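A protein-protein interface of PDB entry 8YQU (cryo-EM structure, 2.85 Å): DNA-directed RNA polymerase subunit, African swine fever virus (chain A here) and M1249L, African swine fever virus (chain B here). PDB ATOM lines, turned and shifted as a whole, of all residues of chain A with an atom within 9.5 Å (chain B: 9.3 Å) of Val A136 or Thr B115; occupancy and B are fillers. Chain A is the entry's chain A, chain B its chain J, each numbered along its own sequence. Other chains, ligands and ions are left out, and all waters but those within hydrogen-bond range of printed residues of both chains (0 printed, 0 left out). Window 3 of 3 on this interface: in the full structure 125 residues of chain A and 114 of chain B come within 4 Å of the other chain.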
ATOM      1  N   ILE A  98      17.835  40.162 -31.219  1.00  0.00           N
ATOM      2  CA  ILE A  98      17.718  38.887 -30.527  1.00  0.00           C
ATOM      3  C   ILE A  98      16.479  38.912 -29.646  1.00  0.00           C
ATOM      4  O   ILE A  98      15.982  39.976 -29.259  1.00  0.00           O
ATOM      5  CB  ILE A  98      18.975  38.579 -29.687  1.00  0.00           C
ATOM      6  CG1 ILE A  98      19.137  39.634 -28.596  1.00  0.00           C
ATOM      7  CG2 ILE A  98      20.210  38.529 -30.572  1.00  0.00           C
ATOM      8  CD1 ILE A  98      20.191  39.308 -27.582  1.00  0.00           C
ATOM      9  N   CYS A  99      15.974  37.725 -29.328  1.00  0.00           N
ATOM     10  CA  CYS A  99      14.886  37.608 -28.370  1.00  0.00           C
ATOM     11  C   CYS A  99      15.423  37.788 -26.955  1.00  0.00           C
ATOM     12  O   CYS A  99      16.540  37.367 -26.640  1.00  0.00           O
ATOM     13  CB  CYS A  99      14.197  36.251 -28.514  1.00  0.00           C
ATOM     14  SG  CYS A  99      12.802  35.999 -27.398  1.00  0.00           S
ATOM     15  N   LEU A 100      14.629  38.424 -26.100  1.00  0.00           N
ATOM     16  CA  LEU A 100      15.052  38.701 -24.733  1.00  0.00           C
ATOM     17  C   LEU A 100      14.766  37.554 -23.772  1.00  0.00           C
ATOM     18  O   LEU A 100      15.077  37.678 -22.584  1.00  0.00           O
ATOM     19  CB  LEU A 100      14.385  39.981 -24.210  1.00  0.00           C
ATOM     20  CG  LEU A 100      15.113  41.320 -24.375  1.00  0.00           C
ATOM     21  CD1 LEU A 100      15.706  41.480 -25.771  1.00  0.00           C
ATOM     22  CD2 LEU A 100      14.189  42.480 -24.033  1.00  0.00           C
ATOM     23  N   ASN A 101      14.187  36.446 -24.246  1.00  0.00           N
ATOM     24  CA  ASN A 101      13.914  35.297 -23.391  1.00  0.00           C
ATOM     25  C   ASN A 101      14.609  34.010 -23.815  1.00  0.00           C
ATOM     26  O   ASN A 101      14.872  33.172 -22.945  1.00  0.00           O
ATOM     27  CB  ASN A 101      12.403  35.024 -23.312  1.00  0.00           C
ATOM     28  CG  ASN A 101      11.656  36.084 -22.524  1.00  0.00           C
ATOM     29  OD1 ASN A 101      12.119  36.539 -21.478  1.00  0.00           O
ATOM     30  ND2 ASN A 101      10.480  36.458 -23.006  1.00  0.00           N
ATOM     31  N   CYS A 102      14.928  33.832 -25.101  1.00  0.00           N
ATOM     32  CA  CYS A 102      15.632  32.638 -25.554  1.00  0.00           C
ATOM     33  C   CYS A 102      16.938  32.959 -26.259  1.00  0.00           C
ATOM     34  O   CYS A 102      17.763  32.055 -26.443  1.00  0.00           O
ATOM     35  CB  CYS A 102      14.795  31.832 -26.544  1.00  0.00           C
ATOM     36  SG  CYS A 102      14.504  32.751 -28.063  1.00  0.00           S
ATOM     37  N   GLY A 103      17.143  34.198 -26.697  1.00  0.00           N
ATOM     38  CA  GLY A 103      18.353  34.608 -27.363  1.00  0.00           C
ATOM     39  C   GLY A 103      18.395  34.371 -28.862  1.00  0.00           C
ATOM     40  O   GLY A 103      19.274  34.930 -29.533  1.00  0.00           O
ATOM     41  N   ALA A 104      17.466  33.594 -29.419  1.00  0.00           N
ATOM     42  CA  ALA A 104      17.509  33.306 -30.845  1.00  0.00           C
ATOM     43  C   ALA A 104      17.235  34.578 -31.649  1.00  0.00           C
ATOM     44  O   ALA A 104      16.523  35.471 -31.184  1.00  0.00           O
ATOM     45  CB  ALA A 104      16.491  32.228 -31.211  1.00  0.00           C
ATOM     46  N   PRO A 105      17.807  34.695 -32.850  1.00  0.00           N
ATOM     47  CA  PRO A 105      17.529  35.880 -33.670  1.00  0.00           C
ATOM     48  C   PRO A 105      16.058  35.945 -34.041  1.00  0.00           C
ATOM     49  O   PRO A 105      15.405  34.923 -34.258  1.00  0.00           O
ATOM     50  CB  PRO A 105      18.416  35.677 -34.903  1.00  0.00           C
ATOM     51  CG  PRO A 105      18.559  34.203 -35.010  1.00  0.00           C
ATOM     52  CD  PRO A 105      18.581  33.686 -33.593  1.00  0.00           C
ATOM     53  N   ILE A 106      15.536  37.165 -34.096  1.00  0.00           N
ATOM     54  CA  ILE A 106      14.142  37.377 -34.468  1.00  0.00           C
ATOM     55  C   ILE A 106      14.006  37.602 -35.964  1.00  0.00           C
ATOM     56  O   ILE A 106      13.188  36.961 -36.629  1.00  0.00           O
ATOM     57  CB  ILE A 106      13.557  38.553 -33.660  1.00  0.00           C
ATOM     58  CG1 ILE A 106      13.325  38.123 -32.213  1.00  0.00           C
ATOM     59  CG2 ILE A 106      12.265  39.041 -34.288  1.00  0.00           C
ATOM     60  CD1 ILE A 106      13.085  39.268 -31.277  1.00  0.00           C
ATOM     61  N   GLN A 133       6.961  37.768 -33.118  1.00  0.00           N
ATOM     62  CA  GLN A 133       6.805  36.587 -32.283  1.00  0.00           C
ATOM     63  C   GLN A 133       7.943  35.608 -32.537  1.00  0.00           C
ATOM     64  O   GLN A 133       8.203  35.217 -33.679  1.00  0.00           O
ATOM     65  CB  GLN A 133       5.450  35.931 -32.559  1.00  0.00           C
ATOM     66  CG  GLN A 133       5.091  34.775 -31.647  1.00  0.00           C
ATOM     67  CD  GLN A 133       5.615  33.452 -32.165  1.00  0.00           C
ATOM     68  OE1 GLN A 133       5.755  33.258 -33.372  1.00  0.00           O
ATOM     69  NE2 GLN A 133       5.911  32.536 -31.254  1.00  0.00           N
ATOM     70  N   CYS A 134       8.624  35.226 -31.461  1.00  0.00           N
ATOM     71  CA  CYS A 134       9.781  34.352 -31.564  1.00  0.00           C
ATOM     72  C   CYS A 134       9.368  32.933 -31.942  1.00  0.00           C
ATOM     73  O   CYS A 134       8.319  32.435 -31.528  1.00  0.00           O
ATOM     74  CB  CYS A 134      10.550  34.339 -30.246  1.00  0.00           C
ATOM     75  SG  CYS A 134      12.142  33.530 -30.363  1.00  0.00           S
ATOM     76  N   TYR A 135      10.223  32.274 -32.722  1.00  0.00           N
ATOM     77  CA  TYR A 135       9.896  30.991 -33.328  1.00  0.00           C
ATOM     78  C   TYR A 135      10.202  29.786 -32.443  1.00  0.00           C
ATOM     79  O   TYR A 135       9.819  28.669 -32.804  1.00  0.00           O
ATOM     80  CB  TYR A 135      10.645  30.828 -34.658  1.00  0.00           C
ATOM     81  CG  TYR A 135      10.145  31.722 -35.770  1.00  0.00           C
ATOM     82  CD1 TYR A 135      10.322  33.099 -35.716  1.00  0.00           C
ATOM     83  CD2 TYR A 135       9.498  31.188 -36.877  1.00  0.00           C
ATOM     84  CE1 TYR A 135       9.865  33.918 -36.729  1.00  0.00           C
ATOM     85  CE2 TYR A 135       9.038  32.000 -37.895  1.00  0.00           C
ATOM     86  CZ  TYR A 135       9.224  33.363 -37.816  1.00  0.00           C
ATOM     87  OH  TYR A 135       8.770  34.176 -38.829  1.00  0.00           O
ATOM     88  N   VAL A 136      10.877  29.968 -31.310  1.00  0.00           N
ATOM     89  CA  VAL A 136      11.333  28.835 -30.515  1.00  0.00           C
ATOM     90  C   VAL A 136      10.876  28.883 -29.062  1.00  0.00           C
ATOM     91  O   VAL A 136      10.842  27.827 -28.410  1.00  0.00           O
ATOM     92  CB  VAL A 136      12.867  28.688 -30.586  1.00  0.00           C
ATOM     93  CG1 VAL A 136      13.277  28.119 -31.932  1.00  0.00           C
ATOM     94  CG2 VAL A 136      13.533  30.028 -30.356  1.00  0.00           C
ATOM     95  N   CYS A 137      10.533  30.051 -28.529  1.00  0.00           N
ATOM     96  CA  CYS A 137      10.065  30.154 -27.155  1.00  0.00           C
ATOM     97  C   CYS A 137       8.669  30.744 -27.041  1.00  0.00           C
ATOM     98  O   CYS A 137       8.086  30.708 -25.951  1.00  0.00           O
ATOM     99  CB  CYS A 137      11.043  30.996 -26.326  1.00  0.00           C
ATOM    100  SG  CYS A 137      10.929  32.761 -26.663  1.00  0.00           S
ATOM    101  N   LYS A 138       8.113  31.265 -28.137  1.00  0.00           N
ATOM    102  CA  LYS A 138       6.782  31.876 -28.153  1.00  0.00           C
ATOM    103  C   LYS A 138       6.723  33.085 -27.219  1.00  0.00           C
ATOM    104  O   LYS A 138       5.970  33.112 -26.244  1.00  0.00           O
ATOM    105  CB  LYS A 138       5.699  30.852 -27.797  1.00  0.00           C
ATOM    106  CG  LYS A 138       5.852  29.503 -28.489  1.00  0.00           C
ATOM    107  CD  LYS A 138       5.580  29.584 -29.978  1.00  0.00           C
ATOM    108  CE  LYS A 138       5.702  28.216 -30.626  1.00  0.00           C
ATOM    109  NZ  LYS A 138       4.636  27.288 -30.164  1.00  0.00           N
ATOM    110  N   ALA A 139       7.538  34.093 -27.521  1.00  0.00           N
ATOM    111  CA  ALA A 139       7.569  35.333 -26.758  1.00  0.00           C
ATOM    112  C   ALA A 139       7.479  36.533 -27.691  1.00  0.00           C
ATOM    113  O   ALA A 139       8.034  36.521 -28.794  1.00  0.00           O
ATOM    114  CB  ALA A 139       8.839  35.434 -25.912  1.00  0.00           C
ATOM    115  N   ARG A 176      23.341  34.544 -23.702  1.00  0.00           N
ATOM    116  CA  ARG A 176      22.556  33.452 -24.272  1.00  0.00           C
ATOM    117  C   ARG A 176      22.591  33.409 -25.794  1.00  0.00           C
ATOM    118  O   ARG A 176      21.967  32.530 -26.393  1.00  0.00           O
ATOM    119  CB  ARG A 176      21.107  33.552 -23.756  1.00  0.00           C
ATOM    120  CG  ARG A 176      20.130  32.463 -24.162  1.00  0.00           C
ATOM    121  CD  ARG A 176      18.783  32.649 -23.545  1.00  0.00           C
ATOM    122  NE  ARG A 176      18.919  32.479 -22.103  1.00  0.00           N
ATOM    123  CZ  ARG A 176      18.768  33.420 -21.185  1.00  0.00           C
ATOM    124  NH1 ARG A 176      18.470  34.670 -21.502  1.00  0.00           N
ATOM    125  NH2 ARG A 176      18.951  33.105 -19.910  1.00  0.00           N
ATOM    126  N   THR A 178      24.355  32.654 -29.340  1.00  0.00           N
ATOM    127  CA  THR A 178      25.347  31.741 -29.880  1.00  0.00           C
ATOM    128  C   THR A 178      26.258  32.448 -30.880  1.00  0.00           C
ATOM    129  O   THR A 178      25.899  33.458 -31.489  1.00  0.00           O
ATOM    130  CB  THR A 178      24.668  30.550 -30.550  1.00  0.00           C
ATOM    131  OG1 THR A 178      23.889  31.004 -31.666  1.00  0.00           O
ATOM    132  CG2 THR A 178      23.763  29.838 -29.567  1.00  0.00           C
ATOM    133  N   ASP A 180      27.053  31.338 -33.719  1.00  0.00           N
ATOM    134  CA  ASP A 180      26.492  31.219 -35.061  1.00  0.00           C
ATOM    135  C   ASP A 180      25.696  32.467 -35.424  1.00  0.00           C
ATOM    136  O   ASP A 180      25.800  32.978 -36.547  1.00  0.00           O
ATOM    137  CB  ASP A 180      25.616  29.967 -35.145  1.00  0.00           C
ATOM    138  CG  ASP A 180      25.191  29.640 -36.563  1.00  0.00           C
ATOM    139  OD1 ASP A 180      25.559  30.393 -37.486  1.00  0.00           O
ATOM    140  OD2 ASP A 180      24.487  28.625 -36.755  1.00  0.00           O
ATOM    141  N   ILE B  91      25.415  20.086 -25.118  1.00  0.00           N
ATOM    142  CA  ILE B  91      24.325  19.361 -24.481  1.00  0.00           C
ATOM    143  C   ILE B  91      23.107  19.354 -25.390  1.00  0.00           C
ATOM    144  O   ILE B  91      22.768  20.373 -26.002  1.00  0.00           O
ATOM    145  CB  ILE B  91      23.968  19.975 -23.108  1.00  0.00           C
ATOM    146  CG1 ILE B  91      25.132  19.829 -22.120  1.00  0.00           C
ATOM    147  CG2 ILE B  91      22.676  19.386 -22.569  1.00  0.00           C
ATOM    148  CD1 ILE B  91      26.118  20.978 -22.136  1.00  0.00           C
ATOM    149  N   VAL B  92      22.460  18.198 -25.493  1.00  0.00           N
ATOM    150  CA  VAL B  92      21.083  18.121 -25.961  1.00  0.00           C
ATOM    151  C   VAL B  92      20.178  18.049 -24.736  1.00  0.00           C
ATOM    152  O   VAL B  92      20.420  17.259 -23.813  1.00  0.00           O
ATOM    153  CB  VAL B  92      20.873  16.920 -26.901  1.00  0.00           C
ATOM    154  CG1 VAL B  92      21.642  17.130 -28.195  1.00  0.00           C
ATOM    155  CG2 VAL B  92      21.318  15.630 -26.246  1.00  0.00           C
ATOM    156  N   SER B  93      19.164  18.906 -24.699  1.00  0.00           N
ATOM    157  CA  SER B  93      18.341  19.086 -23.513  1.00  0.00           C
ATOM    158  C   SER B  93      16.881  18.793 -23.826  1.00  0.00           C
ATOM    159  O   SER B  93      16.365  19.191 -24.875  1.00  0.00           O
ATOM    160  CB  SER B  93      18.481  20.506 -22.959  1.00  0.00           C
ATOM    161  OG  SER B  93      18.034  21.468 -23.898  1.00  0.00           O
ATOM    162  N   GLU B  94      16.225  18.093 -22.904  1.00  0.00           N
ATOM    163  CA  GLU B  94      14.803  17.799 -22.989  1.00  0.00           C
ATOM    164  C   GLU B  94      14.167  18.082 -21.639  1.00  0.00           C
ATOM    165  O   GLU B  94      14.795  17.885 -20.596  1.00  0.00           O
ATOM    166  CB  GLU B  94      14.553  16.342 -23.400  1.00  0.00           C
ATOM    167  CG  GLU B  94      13.082  15.962 -23.532  1.00  0.00           C
ATOM    168  CD  GLU B  94      12.376  16.714 -24.646  1.00  0.00           C
ATOM    169  OE1 GLU B  94      13.050  17.137 -25.608  1.00  0.00           O
ATOM    170  OE2 GLU B  94      11.142  16.882 -24.557  1.00  0.00           O
ATOM    171  N   GLU B 108      26.716  26.746 -25.279  1.00  0.00           N
ATOM    172  CA  GLU B 108      25.904  26.602 -26.478  1.00  0.00           C
ATOM    173  C   GLU B 108      25.460  25.152 -26.606  1.00  0.00           C
ATOM    174  O   GLU B 108      26.290  24.240 -26.632  1.00  0.00           O
ATOM    175  CB  GLU B 108      26.688  27.035 -27.715  1.00  0.00           C
ATOM    176  CG  GLU B 108      27.007  28.519 -27.752  1.00  0.00           C
ATOM    177  CD  GLU B 108      27.797  28.915 -28.983  1.00  0.00           C
ATOM    178  OE1 GLU B 108      28.198  28.018 -29.752  1.00  0.00           O
ATOM    179  OE2 GLU B 108      28.019  30.128 -29.179  1.00  0.00           O
ATOM    180  N   ILE B 109      24.147  24.942 -26.684  1.00  0.00           N
ATOM    181  CA  ILE B 109      23.567  23.611 -26.591  1.00  0.00           C
ATOM    182  C   ILE B 109      22.617  23.371 -27.757  1.00  0.00           C
ATOM    183  O   ILE B 109      22.147  24.299 -28.423  1.00  0.00           O
ATOM    184  CB  ILE B 109      22.824  23.395 -25.254  1.00  0.00           C
ATOM    185  CG1 ILE B 109      21.657  24.373 -25.124  1.00  0.00           C
ATOM    186  CG2 ILE B 109      23.779  23.540 -24.080  1.00  0.00           C
ATOM    187  CD1 ILE B 109      20.744  24.070 -23.959  1.00  0.00           C
ATOM    188  N   PHE B 110      22.357  22.091 -28.000  1.00  0.00           N
ATOM    189  CA  PHE B 110      21.360  21.605 -28.938  1.00  0.00           C
ATOM    190  C   PHE B 110      20.142  21.109 -28.165  1.00  0.00           C
ATOM    191  O   PHE B 110      20.138  21.043 -26.934  1.00  0.00           O
ATOM    192  CB  PHE B 110      21.941  20.494 -29.814  1.00  0.00           C
ATOM    193  CG  PHE B 110      23.002  20.959 -30.769  1.00  0.00           C
ATOM    194  CD1 PHE B 110      22.811  22.091 -31.542  1.00  0.00           C
ATOM    195  CD2 PHE B 110      24.197  20.269 -30.886  1.00  0.00           C
ATOM    196  CE1 PHE B 110      23.787  22.515 -32.422  1.00  0.00           C
ATOM    197  CE2 PHE B 110      25.176  20.692 -31.761  1.00  0.00           C
ATOM    198  CZ  PHE B 110      24.972  21.817 -32.529  1.00  0.00           C
ATOM    199  N   LEU B 111      19.093  20.765 -28.907  1.00  0.00           N
ATOM    200  CA  LEU B 111      17.872  20.228 -28.327  1.00  0.00           C
ATOM    201  C   LEU B 111      17.293  19.194 -29.279  1.00  0.00           C
ATOM    202  O   LEU B 111      17.649  19.136 -30.458  1.00  0.00           O
ATOM    203  CB  LEU B 111      16.832  21.328 -28.057  1.00  0.00           C
ATOM    204  CG  LEU B 111      16.992  22.289 -26.874  1.00  0.00           C
ATOM    205  CD1 LEU B 111      17.932  23.440 -27.202  1.00  0.00           C
ATOM    206  CD2 LEU B 111      15.635  22.820 -26.436  1.00  0.00           C
ATOM    207  N   ILE B 112      16.395  18.361 -28.754  1.00  0.00           N
ATOM    208  CA  ILE B 112      15.526  17.584 -29.625  1.00  0.00           C
ATOM    209  C   ILE B 112      14.591  18.545 -30.345  1.00  0.00           C
ATOM    210  O   ILE B 112      14.119  19.530 -29.760  1.00  0.00           O
ATOM    211  CB  ILE B 112      14.761  16.517 -28.825  1.00  0.00           C
ATOM    212  CG1 ILE B 112      15.746  15.599 -28.099  1.00  0.00           C
ATOM    213  CG2 ILE B 112      13.857  15.700 -29.736  1.00  0.00           C
ATOM    214  CD1 ILE B 112      15.906  15.893 -26.632  1.00  0.00           C
ATOM    215  N   ASN B 113      14.327  18.260 -31.622  1.00  0.00           N
ATOM    216  CA  ASN B 113      13.803  19.135 -32.668  1.00  0.00           C
ATOM    217  C   ASN B 113      14.955  19.975 -33.233  1.00  0.00           C
ATOM    218  O   ASN B 113      14.745  20.741 -34.173  1.00  0.00           O
ATOM    219  CB  ASN B 113      12.658  20.055 -32.188  1.00  0.00           C
ATOM    220  CG  ASN B 113      11.916  20.747 -33.326  1.00  0.00           C
ATOM    221  OD1 ASN B 113      12.225  20.566 -34.503  1.00  0.00           O
ATOM    222  ND2 ASN B 113      10.925  21.555 -32.967  1.00  0.00           N
ATOM    223  N   GLY B 114      16.171  19.836 -32.707  1.00  0.00           N
ATOM    224  CA  GLY B 114      17.358  20.396 -33.320  1.00  0.00           C
ATOM    225  C   GLY B 114      17.462  21.905 -33.400  1.00  0.00           C
ATOM    226  O   GLY B 114      17.802  22.446 -34.455  1.00  0.00           O
ATOM    227  N   THR B 115      17.177  22.597 -32.303  1.00  0.00           N
ATOM    228  CA  THR B 115      17.366  24.039 -32.234  1.00  0.00           C
ATOM    229  C   THR B 115      18.649  24.360 -31.474  1.00  0.00           C
ATOM    230  O   THR B 115      18.916  23.797 -30.409  1.00  0.00           O
ATOM    231  CB  THR B 115      16.161  24.724 -31.579  1.00  0.00           C
ATOM    232  OG1 THR B 115      16.399  26.134 -31.483  1.00  0.00           O
ATOM    233  CG2 THR B 115      15.875  24.149 -30.197  1.00  0.00           C
ATOM    234  N   HIS B 116      19.454  25.253 -32.046  1.00  0.00           N
ATOM    235  CA  HIS B 116      20.733  25.645 -31.461  1.00  0.00           C
ATOM    236  C   HIS B 116      20.518  26.870 -30.582  1.00  0.00           C
ATOM    237  O   HIS B 116      20.239  27.963 -31.085  1.00  0.00           O
ATOM    238  CB  HIS B 116      21.762  25.919 -32.556  1.00  0.00           C
ATOM    239  CG  HIS B 116      23.111  26.309 -32.037  1.00  0.00           C
ATOM    240  ND1 HIS B 116      23.972  25.410 -31.446  1.00  0.00           N
ATOM    241  CD2 HIS B 116      23.756  27.499 -32.042  1.00  0.00           C
ATOM    242  CE1 HIS B 116      25.083  26.032 -31.096  1.00  0.00           C
ATOM    243  NE2 HIS B 116      24.979  27.301 -31.447  1.00  0.00           N
ATOM    244  N   LEU B 117      20.651  26.689 -29.270  1.00  0.00           N
ATOM    245  CA  LEU B 117      20.443  27.756 -28.304  1.00  0.00           C
ATOM    246  C   LEU B 117      21.678  27.853 -27.417  1.00  0.00           C
ATOM    247  O   LEU B 117      22.692  27.197 -27.660  1.00  0.00           O
ATOM    248  CB  LEU B 117      19.182  27.506 -27.468  1.00  0.00           C
ATOM    249  CG  LEU B 117      17.847  27.590 -28.212  1.00  0.00           C
ATOM    250  CD1 LEU B 117      16.705  27.102 -27.334  1.00  0.00           C
ATOM    251  CD2 LEU B 117      17.584  29.005 -28.701  1.00  0.00           C
ATOM    252  N   ALA B 118      21.594  28.683 -26.382  1.00  0.00           N
ATOM    253  CA  ALA B 118      22.639  28.759 -25.372  1.00  0.00           C
ATOM    254  C   ALA B 118      21.997  28.928 -24.004  1.00  0.00           C
ATOM    255  O   ALA B 118      20.803  29.208 -23.883  1.00  0.00           O
ATOM    256  CB  ALA B 118      23.628  29.897 -25.647  1.00  0.00           C
ATOM    257  N   TRP B 181      21.131  10.100 -33.488  1.00  0.00           N
ATOM    258  CA  TRP B 181      20.908  11.528 -33.650  1.00  0.00           C
ATOM    259  C   TRP B 181      21.898  12.044 -34.685  1.00  0.00           C
ATOM    260  O   TRP B 181      23.019  11.541 -34.803  1.00  0.00           O
ATOM    261  CB  TRP B 181      21.046  12.256 -32.307  1.00  0.00           C
ATOM    262  CG  TRP B 181      20.751  13.719 -32.347  1.00  0.00           C
ATOM    263  CD1 TRP B 181      19.555  14.300 -32.647  1.00  0.00           C
ATOM    264  CD2 TRP B 181      21.646  14.788 -32.024  1.00  0.00           C
ATOM    265  NE1 TRP B 181      19.655  15.666 -32.556  1.00  0.00           N
ATOM    266  CE2 TRP B 181      20.929  15.992 -32.174  1.00  0.00           C
ATOM    267  CE3 TRP B 181      22.988  14.846 -31.635  1.00  0.00           C
ATOM    268  CZ2 TRP B 181      21.507  17.237 -31.947  1.00  0.00           C
ATOM    269  CZ3 TRP B 181      23.558  16.085 -31.412  1.00  0.00           C
ATOM    270  CH2 TRP B 181      22.820  17.262 -31.571  1.00  0.00           C
ATOM    271  N   LYS B 182      21.474  13.055 -35.441  1.00  0.00           N
ATOM    272  CA  LYS B 182      22.197  13.445 -36.645  1.00  0.00           C
ATOM    273  C   LYS B 182      22.193  14.956 -36.807  1.00  0.00           C
ATOM    274  O   LYS B 182      21.132  15.584 -36.746  1.00  0.00           O
ATOM    275  CB  LYS B 182      21.571  12.788 -37.880  1.00  0.00           C
ATOM    276  CG  LYS B 182      20.050  12.784 -37.853  1.00  0.00           C
ATOM    277  CD  LYS B 182      19.468  11.652 -38.677  1.00  0.00           C
ATOM    278  CE  LYS B 182      17.950  11.697 -38.658  1.00  0.00           C
ATOM    279  NZ  LYS B 182      17.423  12.944 -39.277  1.00  0.00           N
ATOM    280  N   LYS B 183      23.376  15.527 -37.030  1.00  0.00           N
ATOM    281  CA  LYS B 183      23.542  16.944 -37.344  1.00  0.00           C
ATOM    282  C   LYS B 183      24.694  17.098 -38.331  1.00  0.00           C
ATOM    283  O   LYS B 183      25.135  16.128 -38.958  1.00  0.00           O
ATOM    284  CB  LYS B 183      23.764  17.790 -36.082  1.00  0.00           C
ATOM    285  CG  LYS B 183      22.583  17.814 -35.142  1.00  0.00           C
ATOM    286  CD  LYS B 183      21.439  18.546 -35.823  1.00  0.00           C
ATOM    287  CE  LYS B 183      20.219  18.680 -34.943  1.00  0.00           C
ATOM    288  NZ  LYS B 183      19.135  19.365 -35.698  1.00  0.00           N
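N of Ala A104 sits close to SG of Cys A102 (3.4 Å). The backbone carbonyl oxygen of Leu B117 lies within hydrogen-bond range of the backbone NH of Ile B109.
Among the printed residues, pairs that only touch across the chains: Thr A178 with Glu B108 (3.2 Å), Arg A176 with Ala B118 (3.2 Å), Thr A178 with His B116 (3.4 Å), Thr A178 with Leu B117 (3.4 Å), Val A136 with Thr B115 (3.7 Å), Cys A102 with Leu B117 (3.8 Å) and Thr A178 with Ala B118 (3.9 Å).
Of chain B, only Thr B115 (3.7 Å) comes within 4 Å of Val A136. Thr B115 touches one residue of chain A. No residue of chain B comes within 4 Å of Cys A137. No residue of chain A comes within 4 Å of Leu B111. No residue of chain A comes within 4 Å of Gly B114. Of the printed residues of chain B, Arg A176 touches Ala B118. Printed residues of chain A within 4 Å of Leu B117: Cys A102 and Thr A178. Of the printed residues of chain A, Glu B108 touches Thr A178 (3.2 Å). Asn B113 touches none of the printed residues of chain A. The nearest residue of chain B that does not touch Val A136 is Leu B117 (4.5 Å). The nearest residue of chain A that does not touch Thr B115 is Ala A104 (6.1 Å).
Among the printed residues, 7 pairs touch across the chains.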
